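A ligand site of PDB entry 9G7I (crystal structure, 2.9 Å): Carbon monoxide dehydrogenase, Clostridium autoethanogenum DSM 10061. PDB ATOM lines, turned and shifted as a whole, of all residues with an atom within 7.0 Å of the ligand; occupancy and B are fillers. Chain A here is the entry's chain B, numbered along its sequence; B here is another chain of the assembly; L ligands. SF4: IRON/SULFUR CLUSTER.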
ATOM      1  N   CYS A  46     -19.630 -15.912   0.412  1.00  0.00           N
ATOM      2  CA  CYS A  46     -19.924 -16.846  -0.671  1.00  0.00           C
ATOM      3  C   CYS A  46     -21.056 -16.234  -1.480  1.00  0.00           C
ATOM      4  O   CYS A  46     -22.065 -15.830  -0.891  1.00  0.00           O
ATOM      5  CB  CYS A  46     -20.312 -18.212  -0.115  1.00  0.00           C
ATOM      6  SG  CYS A  46     -20.806 -19.396  -1.390  1.00  0.00           S
ATOM      7  N   CYS A  47     -20.904 -16.145  -2.806  1.00  0.00           N
ATOM      8  CA  CYS A  47     -21.937 -15.547  -3.647  1.00  0.00           C
ATOM      9  C   CYS A  47     -22.481 -16.518  -4.685  1.00  0.00           C
ATOM     10  O   CYS A  47     -21.702 -17.181  -5.370  1.00  0.00           O
ATOM     11  CB  CYS A  47     -21.414 -14.289  -4.318  1.00  0.00           C
ATOM     12  SG  CYS A  47     -22.681 -13.363  -5.218  1.00  0.00           S
ATOM     13  N   ARG A  48     -23.811 -16.588  -4.814  1.00  0.00           N
ATOM     14  CA  ARG A  48     -24.482 -17.438  -5.788  1.00  0.00           C
ATOM     15  C   ARG A  48     -25.578 -16.625  -6.477  1.00  0.00           C
ATOM     16  O   ARG A  48     -26.677 -17.124  -6.692  1.00  0.00           O
ATOM     17  CB  ARG A  48     -25.079 -18.684  -5.114  1.00  0.00           C
ATOM     18  CG  ARG A  48     -24.045 -19.606  -4.481  1.00  0.00           C
ATOM     19  CD  ARG A  48     -24.585 -21.008  -4.228  1.00  0.00           C
ATOM     20  NE  ARG A  48     -24.850 -21.245  -2.802  1.00  0.00           N
ATOM     21  CZ  ARG A  48     -25.996 -20.967  -2.165  1.00  0.00           C
ATOM     22  NH1 ARG A  48     -27.012 -20.425  -2.822  1.00  0.00           N
ATOM     23  NH2 ARG A  48     -26.126 -21.233  -0.870  1.00  0.00           N
ATOM     24  N   ASN A  49     -25.260 -15.387  -6.866  1.00  0.00           N
ATOM     25  CA  ASN A  49     -26.279 -14.496  -7.475  1.00  0.00           C
ATOM     26  C   ASN A  49     -26.252 -14.623  -9.008  1.00  0.00           C
ATOM     27  O   ASN A  49     -27.040 -13.931  -9.664  1.00  0.00           O
ATOM     28  CB  ASN A  49     -26.101 -13.041  -7.026  1.00  0.00           C
ATOM     29  CG  ASN A  49     -26.529 -12.818  -5.592  1.00  0.00           C
ATOM     30  OD1 ASN A  49     -26.366 -13.696  -4.744  1.00  0.00           O
ATOM     31  ND2 ASN A  49     -27.063 -11.644  -5.307  1.00  0.00           N
ATOM     32  N   CYS A  50     -25.382 -15.485  -9.541  1.00  0.00           N
ATOM     33  CA  CYS A  50     -25.385 -15.724 -11.003  1.00  0.00           C
ATOM     34  C   CYS A  50     -24.721 -17.075 -11.297  1.00  0.00           C
ATOM     35  O   CYS A  50     -24.022 -17.586 -10.400  1.00  0.00           O
ATOM     36  CB  CYS A  50     -24.716 -14.581 -11.762  1.00  0.00           C
ATOM     37  SG  CYS A  50     -22.914 -14.661 -11.711  1.00  0.00           S
ATOM     38  N   SER A  51     -24.921 -17.604 -12.505  1.00  0.00           N
ATOM     39  CA  SER A  51     -24.399 -18.965 -12.848  1.00  0.00           C
ATOM     40  C   SER A  51     -22.915 -18.913 -13.223  1.00  0.00           C
ATOM     41  O   SER A  51     -22.378 -19.963 -13.606  1.00  0.00           O
ATOM     42  CB  SER A  51     -25.227 -19.577 -13.946  1.00  0.00           C
ATOM     43  OG  SER A  51     -24.644 -19.325 -15.218  1.00  0.00           O
ATOM     44  N   MET A  52     -22.304 -17.727 -13.186  1.00  0.00           N
ATOM     45  CA  MET A  52     -20.837 -17.660 -13.405  1.00  0.00           C
ATOM     46  C   MET A  52     -20.234 -18.280 -12.150  1.00  0.00           C
ATOM     47  O   MET A  52     -19.123 -18.823 -12.230  1.00  0.00           O
ATOM     48  CB  MET A  52     -20.362 -16.218 -13.616  1.00  0.00           C
ATOM     49  CG  MET A  52     -20.844 -15.612 -14.918  1.00  0.00           C
ATOM     50  SD  MET A  52     -19.734 -14.318 -15.529  1.00  0.00           S
ATOM     51  CE  MET A  52     -19.946 -13.064 -14.278  1.00  0.00           C
ATOM     52  N   GLY A  53     -20.981 -18.211 -11.040  1.00  0.00           N
ATOM     53  CA  GLY A  53     -20.511 -18.792  -9.769  1.00  0.00           C
ATOM     54  C   GLY A  53     -20.796 -20.278  -9.654  1.00  0.00           C
ATOM     55  O   GLY A  53     -21.198 -20.875 -10.667  1.00  0.00           O
ATOM     56  N   PRO A  54     -20.618 -20.911  -8.470  1.00  0.00           N
ATOM     57  CA  PRO A  54     -20.521 -20.197  -7.198  1.00  0.00           C
ATOM     58  C   PRO A  54     -19.143 -19.536  -7.006  1.00  0.00           C
ATOM     59  O   PRO A  54     -18.191 -19.996  -7.593  1.00  0.00           O
ATOM     60  CB  PRO A  54     -20.680 -21.297  -6.134  1.00  0.00           C
ATOM     61  CG  PRO A  54     -21.119 -22.529  -6.907  1.00  0.00           C
ATOM     62  CD  PRO A  54     -20.520 -22.363  -8.284  1.00  0.00           C
ATOM     63  N   CYS A  55     -19.088 -18.476  -6.189  1.00  0.00           N
ATOM     64  CA  CYS A  55     -17.783 -17.804  -5.903  1.00  0.00           C
ATOM     65  C   CYS A  55     -17.577 -17.697  -4.386  1.00  0.00           C
ATOM     66  O   CYS A  55     -18.590 -17.524  -3.673  1.00  0.00           O
ATOM     67  CB  CYS A  55     -17.745 -16.417  -6.529  1.00  0.00           C
ATOM     68  SG  CYS A  55     -18.227 -16.381  -8.276  1.00  0.00           S
ATOM     69  N   ARG A  56     -16.334 -17.785  -3.923  1.00  0.00           N
ATOM     70  CA  ARG A  56     -16.016 -17.682  -2.468  1.00  0.00           C
ATOM     71  C   ARG A  56     -14.723 -16.899  -2.279  1.00  0.00           C
ATOM     72  O   ARG A  56     -13.648 -17.448  -2.570  1.00  0.00           O
ATOM     73  CB  ARG A  56     -15.978 -19.058  -1.790  1.00  0.00           C
ATOM     74  CG  ARG A  56     -15.121 -20.105  -2.473  1.00  0.00           C
ATOM     75  CD  ARG A  56     -15.268 -21.416  -1.715  1.00  0.00           C
ATOM     76  NE  ARG A  56     -14.765 -22.497  -2.542  1.00  0.00           N
ATOM     77  CZ  ARG A  56     -14.980 -23.732  -2.137  1.00  0.00           C
ATOM     78  NH1 ARG A  56     -15.649 -23.918  -1.010  1.00  0.00           N
ATOM     79  NH2 ARG A  56     -14.534 -24.768  -2.830  1.00  0.00           N
ATOM     80  N   VAL A  57     -14.834 -15.659  -1.807  1.00  0.00           N
ATOM     81  CA  VAL A  57     -13.642 -14.790  -1.565  1.00  0.00           C
ATOM     82  C   VAL A  57     -13.148 -15.021  -0.126  1.00  0.00           C
ATOM     83  O   VAL A  57     -13.850 -15.725   0.623  1.00  0.00           O
ATOM     84  CB  VAL A  57     -13.959 -13.302  -1.815  1.00  0.00           C
ATOM     85  CG1 VAL A  57     -14.176 -13.022  -3.294  1.00  0.00           C
ATOM     86  CG2 VAL A  57     -15.153 -12.841  -1.003  1.00  0.00           C
ATOM     87  N   ARG A  67     -11.567 -11.094  -5.296  1.00  0.00           N
ATOM     88  CA  ARG A  67     -12.842 -10.704  -5.911  1.00  0.00           C
ATOM     89  C   ARG A  67     -13.548 -11.892  -6.577  1.00  0.00           C
ATOM     90  O   ARG A  67     -12.932 -12.925  -6.852  1.00  0.00           O
ATOM     91  CB  ARG A  67     -12.604  -9.605  -6.972  1.00  0.00           C
ATOM     92  CG  ARG A  67     -11.758  -8.424  -6.469  1.00  0.00           C
ATOM     93  CD  ARG A  67     -11.159  -7.592  -7.597  1.00  0.00           C
ATOM     94  NE  ARG A  67     -12.008  -6.432  -7.915  1.00  0.00           N
ATOM     95  CZ  ARG A  67     -11.913  -5.239  -7.349  1.00  0.00           C
ATOM     96  NH1 ARG A  67     -11.004  -5.008  -6.399  1.00  0.00           N
ATOM     97  NH2 ARG A  67     -12.733  -4.251  -7.714  1.00  0.00           N
ATOM     98  N   GLY A  68     -14.846 -11.735  -6.838  1.00  0.00           N
ATOM     99  CA  GLY A  68     -15.649 -12.754  -7.496  1.00  0.00           C
ATOM    100  C   GLY A  68     -15.391 -12.791  -8.985  1.00  0.00           C
ATOM    101  O   GLY A  68     -14.575 -12.013  -9.491  1.00  0.00           O
ATOM    102  N   ILE A  69     -16.122 -13.612  -9.738  1.00  0.00           N
ATOM    103  CA  ILE A  69     -15.811 -13.694 -11.197  1.00  0.00           C
ATOM    104  C   ILE A  69     -16.197 -12.363 -11.854  1.00  0.00           C
ATOM    105  O   ILE A  69     -15.462 -11.916 -12.748  1.00  0.00           O
ATOM    106  CB  ILE A  69     -16.480 -14.923 -11.831  1.00  0.00           C
ATOM    107  CG1 ILE A  69     -15.874 -16.210 -11.289  1.00  0.00           C
ATOM    108  CG2 ILE A  69     -16.427 -14.855 -13.350  1.00  0.00           C
ATOM    109  CD1 ILE A  69     -16.388 -17.460 -11.957  1.00  0.00           C
ATOM    110  N   CYS A  70     -17.310 -11.744 -11.426  1.00  0.00           N
ATOM    111  CA  CYS A  70     -17.708 -10.440 -11.945  1.00  0.00           C
ATOM    112  C   CYS A  70     -16.816  -9.288 -11.462  1.00  0.00           C
ATOM    113  O   CYS A  70     -16.900  -8.187 -12.016  1.00  0.00           O
ATOM    114  CB  CYS A  70     -19.174 -10.170 -11.619  1.00  0.00           C
ATOM    115  SG  CYS A  70     -19.546 -10.152  -9.838  1.00  0.00           S
ATOM    116  N   GLY A  71     -15.984  -9.528 -10.451  1.00  0.00           N
ATOM    117  CA  GLY A  71     -15.105  -8.507  -9.882  1.00  0.00           C
ATOM    118  C   GLY A  71     -15.597  -7.951  -8.572  1.00  0.00           C
ATOM    119  O   GLY A  71     -15.042  -6.970  -8.062  1.00  0.00           O
ATOM    120  N   ALA A  72     -16.649  -8.568  -7.987  1.00  0.00           N
ATOM    121  CA  ALA A  72     -17.240  -8.124  -6.725  1.00  0.00           C
ATOM    122  C   ALA A  72     -16.318  -8.397  -5.536  1.00  0.00           C
ATOM    123  O   ALA A  72     -15.914  -9.533  -5.306  1.00  0.00           O
ATOM    124  CB  ALA A  72     -18.568  -8.826  -6.502  1.00  0.00           C
ATOM    125  N   ILE A  77     -20.118  -8.573  -1.778  1.00  0.00           N
ATOM    126  CA  ILE A  77     -20.741  -9.881  -1.573  1.00  0.00           C
ATOM    127  C   ILE A  77     -21.474  -9.967  -0.234  1.00  0.00           C
ATOM    128  O   ILE A  77     -22.645 -10.335  -0.196  1.00  0.00           O
ATOM    129  CB  ILE A  77     -19.698 -11.023  -1.722  1.00  0.00           C
ATOM    130  CG1 ILE A  77     -19.166 -11.088  -3.164  1.00  0.00           C
ATOM    131  CG2 ILE A  77     -20.290 -12.363  -1.288  1.00  0.00           C
ATOM    132  CD1 ILE A  77     -17.784 -11.670  -3.296  1.00  0.00           C
ATOM    133  N   ARG A  80     -24.551  -7.569  -0.087  1.00  0.00           N
ATOM    134  CA  ARG A  80     -25.660  -8.027  -0.904  1.00  0.00           C
ATOM    135  C   ARG A  80     -26.360  -9.190  -0.206  1.00  0.00           C
ATOM    136  O   ARG A  80     -27.585  -9.256  -0.198  1.00  0.00           O
ATOM    137  CB  ARG A  80     -25.184  -8.464  -2.304  1.00  0.00           C
ATOM    138  CG  ARG A  80     -24.587  -7.319  -3.109  1.00  0.00           C
ATOM    139  CD  ARG A  80     -24.371  -7.653  -4.571  1.00  0.00           C
ATOM    140  NE  ARG A  80     -23.494  -8.806  -4.768  1.00  0.00           N
ATOM    141  CZ  ARG A  80     -22.997  -9.184  -5.940  1.00  0.00           C
ATOM    142  NH1 ARG A  80     -23.281  -8.485  -7.040  1.00  0.00           N
ATOM    143  NH2 ARG A  80     -22.213 -10.251  -6.034  1.00  0.00           N
ATOM    144  N   THR A 194     -29.272  -6.170  -5.814  1.00  0.00           N
ATOM    145  CA  THR A 194     -28.418  -7.293  -5.422  1.00  0.00           C
ATOM    146  C   THR A 194     -28.102  -8.204  -6.628  1.00  0.00           C
ATOM    147  O   THR A 194     -27.190  -9.017  -6.549  1.00  0.00           O
ATOM    148  CB  THR A 194     -29.067  -8.092  -4.281  1.00  0.00           C
ATOM    149  OG1 THR A 194     -30.414  -8.420  -4.645  1.00  0.00           O
ATOM    150  CG2 THR A 194     -29.012  -7.363  -2.944  1.00  0.00           C
ATOM    151  N   HIS A 195     -28.847  -8.056  -7.740  1.00  0.00           N
ATOM    152  CA  HIS A 195     -28.617  -8.846  -8.949  1.00  0.00           C
ATOM    153  C   HIS A 195     -27.230  -8.529  -9.511  1.00  0.00           C
ATOM    154  O   HIS A 195     -26.723  -7.426  -9.311  1.00  0.00           O
ATOM    155  CB  HIS A 195     -29.719  -8.563  -9.987  1.00  0.00           C
ATOM    156  CG  HIS A 195     -29.521  -9.223 -11.322  1.00  0.00           C
ATOM    157  ND1 HIS A 195     -29.107 -10.538 -11.429  1.00  0.00           N
ATOM    158  CD2 HIS A 195     -29.726  -8.725 -12.561  1.00  0.00           C
ATOM    159  CE1 HIS A 195     -29.031 -10.783 -12.731  1.00  0.00           C
ATOM    160  NE2 HIS A 195     -29.416  -9.721 -13.452  1.00  0.00           N
ATOM    161  N   ILE A 196     -26.668  -9.491 -10.247  1.00  0.00           N
ATOM    162  CA  ILE A 196     -25.299  -9.326 -10.799  1.00  0.00           C
ATOM    163  C   ILE A 196     -25.195  -8.056 -11.637  1.00  0.00           C
ATOM    164  O   ILE A 196     -26.160  -7.730 -12.345  1.00  0.00           O
ATOM    165  CB  ILE A 196     -24.887 -10.580 -11.610  1.00  0.00           C
ATOM    166  CG1 ILE A 196     -23.373 -10.714 -11.718  1.00  0.00           C
ATOM    167  CG2 ILE A 196     -25.562 -10.592 -12.965  1.00  0.00           C
ATOM    168  CD1 ILE A 196     -22.785 -10.043 -12.942  1.00  0.00           C
ATOM    169  N   GLY A 197     -24.066  -7.355 -11.516  1.00  0.00           N
ATOM    170  CA  GLY A 197     -23.803  -6.161 -12.303  1.00  0.00           C
ATOM    171  C   GLY A 197     -24.575  -4.927 -11.893  1.00  0.00           C
ATOM    172  O   GLY A 197     -24.735  -4.016 -12.709  1.00  0.00           O
ATOM    173  N   VAL B  27     -12.250 -11.079 -16.528  1.00  0.00           N
ATOM    174  CA  VAL B  27     -13.205 -12.091 -16.054  1.00  0.00           C
ATOM    175  C   VAL B  27     -12.644 -13.512 -16.271  1.00  0.00           C
ATOM    176  O   VAL B  27     -12.850 -14.381 -15.421  1.00  0.00           O
ATOM    177  CB  VAL B  27     -14.578 -11.896 -16.743  1.00  0.00           C
ATOM    178  CG1 VAL B  27     -14.484 -12.086 -18.251  1.00  0.00           C
ATOM    179  CG2 VAL B  27     -15.635 -12.808 -16.140  1.00  0.00           C
ATOM    180  N   MET B  34     -10.780 -18.756  -9.309  1.00  0.00           N
ATOM    181  CA  MET B  34     -11.812 -19.444  -8.524  1.00  0.00           C
ATOM    182  C   MET B  34     -11.552 -20.953  -8.440  1.00  0.00           C
ATOM    183  O   MET B  34     -12.047 -21.596  -7.515  1.00  0.00           O
ATOM    184  CB  MET B  34     -13.216 -19.194  -9.118  1.00  0.00           C
ATOM    185  CG  MET B  34     -13.999 -18.077  -8.424  1.00  0.00           C
ATOM    186  SD  MET B  34     -14.101 -18.212  -6.618  1.00  0.00           S
ATOM    187  CE  MET B  34     -14.825 -19.852  -6.466  1.00  0.00           C
ATOM    188  N   GLN B  37     -15.123 -25.092  -8.335  1.00  0.00           N
ATOM    189  CA  GLN B  37     -16.238 -24.316  -7.738  1.00  0.00           C
ATOM    190  C   GLN B  37     -17.009 -25.236  -6.785  1.00  0.00           C
ATOM    191  O   GLN B  37     -17.131 -26.435  -7.107  1.00  0.00           O
ATOM    192  CB  GLN B  37     -17.126 -23.716  -8.835  1.00  0.00           C
ATOM    193  CG  GLN B  37     -16.460 -22.586  -9.599  1.00  0.00           C
ATOM    194  CD  GLN B  37     -17.479 -21.769 -10.364  1.00  0.00           C
ATOM    195  OE1 GLN B  37     -18.363 -22.332 -11.003  1.00  0.00           O
ATOM    196  NE2 GLN B  37     -17.376 -20.448 -10.317  1.00  0.00           N
ATOM    197  N   PRO B 336     -18.353  -5.108 -11.649  1.00  0.00           N
ATOM    198  CA  PRO B 336     -17.678  -4.132 -10.760  1.00  0.00           C
ATOM    199  C   PRO B 336     -16.172  -3.990 -11.010  1.00  0.00           C
ATOM    200  O   PRO B 336     -15.585  -3.021 -10.529  1.00  0.00           O
ATOM    201  CB  PRO B 336     -17.953  -4.663  -9.352  1.00  0.00           C
ATOM    202  CG  PRO B 336     -19.085  -5.604  -9.490  1.00  0.00           C
ATOM    203  CD  PRO B 336     -19.026  -6.162 -10.871  1.00  0.00           C
ATOM    204  N   MET B 557     -25.985 -16.516 -17.490  1.00  0.00           N
ATOM    205  CA  MET B 557     -25.517 -16.389 -16.116  1.00  0.00           C
ATOM    206  C   MET B 557     -26.597 -15.671 -15.322  1.00  0.00           C
ATOM    207  O   MET B 557     -27.088 -16.197 -14.339  1.00  0.00           O
ATOM    208  CB  MET B 557     -24.089 -15.795 -16.055  1.00  0.00           C
ATOM    209  CG  MET B 557     -23.837 -14.611 -16.976  1.00  0.00           C
ATOM    210  SD  MET B 557     -24.562 -13.045 -16.425  1.00  0.00           S
ATOM    211  CE  MET B 557     -23.456 -12.606 -15.171  1.00  0.00           C
HETATM  212 FE1  SF4 L   1     -19.607 -14.803  -8.983  1.00  0.00          FE
HETATM  213 FE2  SF4 L   1     -20.097 -12.192  -8.783  1.00  0.00          FE
HETATM  214 FE3  SF4 L   1     -21.338 -13.927  -7.179  1.00  0.00          FE
HETATM  215 FE4  SF4 L   1     -21.970 -13.865  -9.705  1.00  0.00          FE
HETATM  216  S1  SF4 L   1     -22.335 -12.143  -8.219  1.00  0.00           S
HETATM  217  S2  SF4 L   1     -21.649 -15.778  -8.498  1.00  0.00           S
HETATM  218  S3  SF4 L   1     -19.968 -13.400 -10.760  1.00  0.00           S
HETATM  219  S4  SF4 L   1     -19.062 -13.450  -7.174  1.00  0.00           S
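An iron atom (FE1) of the ligand is bound by the side-chain sulfur (SG) of Cys 55 (2.2 Å).
An iron atom (FE4) of the ligand is bound by the side-chain sulfur (SG) of Cys 50, at 2.4 Å.
S3 of the ligand sits close to N of Cys 70 (3.2 Å).
FE2 of the ligand is bound by SG of Cys 70, at 2.4 Å.
The side-chain sulfur (SG) of Cys 47 binds an iron atom (FE3) of the ligand (2.4 Å).
The guanidinium group of Arg 80 lies close to a sulfur (S1) of the ligand, at 2.9 Å.
The backbone NH of Gly 53 sits close to a sulfur (S2) of the ligand, at 3.6 Å.
O of Cys 55 is in hydrogen-bond range of N of Cys 47 (2.8 Å).
The backbone NH (N) of Met 52 lies close to the side-chain sulfur (SG) of Cys 50 (3.5 Å).
SG of Cys 70 sits close to N of Ala 72 (3.8 Å).
NH2 of Arg 80 lies close to SG of Cys 47, at 3.3 Å.
N of Asn 49 sits close to SG of Cys 47.
OE1 of Gln 37 of chain B lies close to O of Gly 53 (3.2 Å).
O of Met 52 is in hydrogen-bond range of NE2 of Gln 37 of chain B (3.1 Å).
The side-chain amide nitrogen of Asn 49 lies within hydrogen-bond range of the backbone carbonyl oxygen of Thr 194 (2.9 Å).
N of Asn 49 touches S2 of the ligand, 3.98 Å away.
Met 52 touches the ligand.
CA of Gly 68 touches S4 of the ligand (3.5 Å).
Ile 69 touches the ligand (N to FE1, 3.8 Å).
CG1 of Ile 196 touches S1 of the ligand, 3.9 Å away.
Hydrophobic or aromatic side chains that line the ligand: Met 52, Ile 69 and Ile 196.
11 residues have an atom within 4 Å of the ligand: Cys 47, Asn 49, Cys 50, Met 52, Gly 53, Cys 55, Gly 68, Ile 69, Cys 70, Arg 80 and Ile 196.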
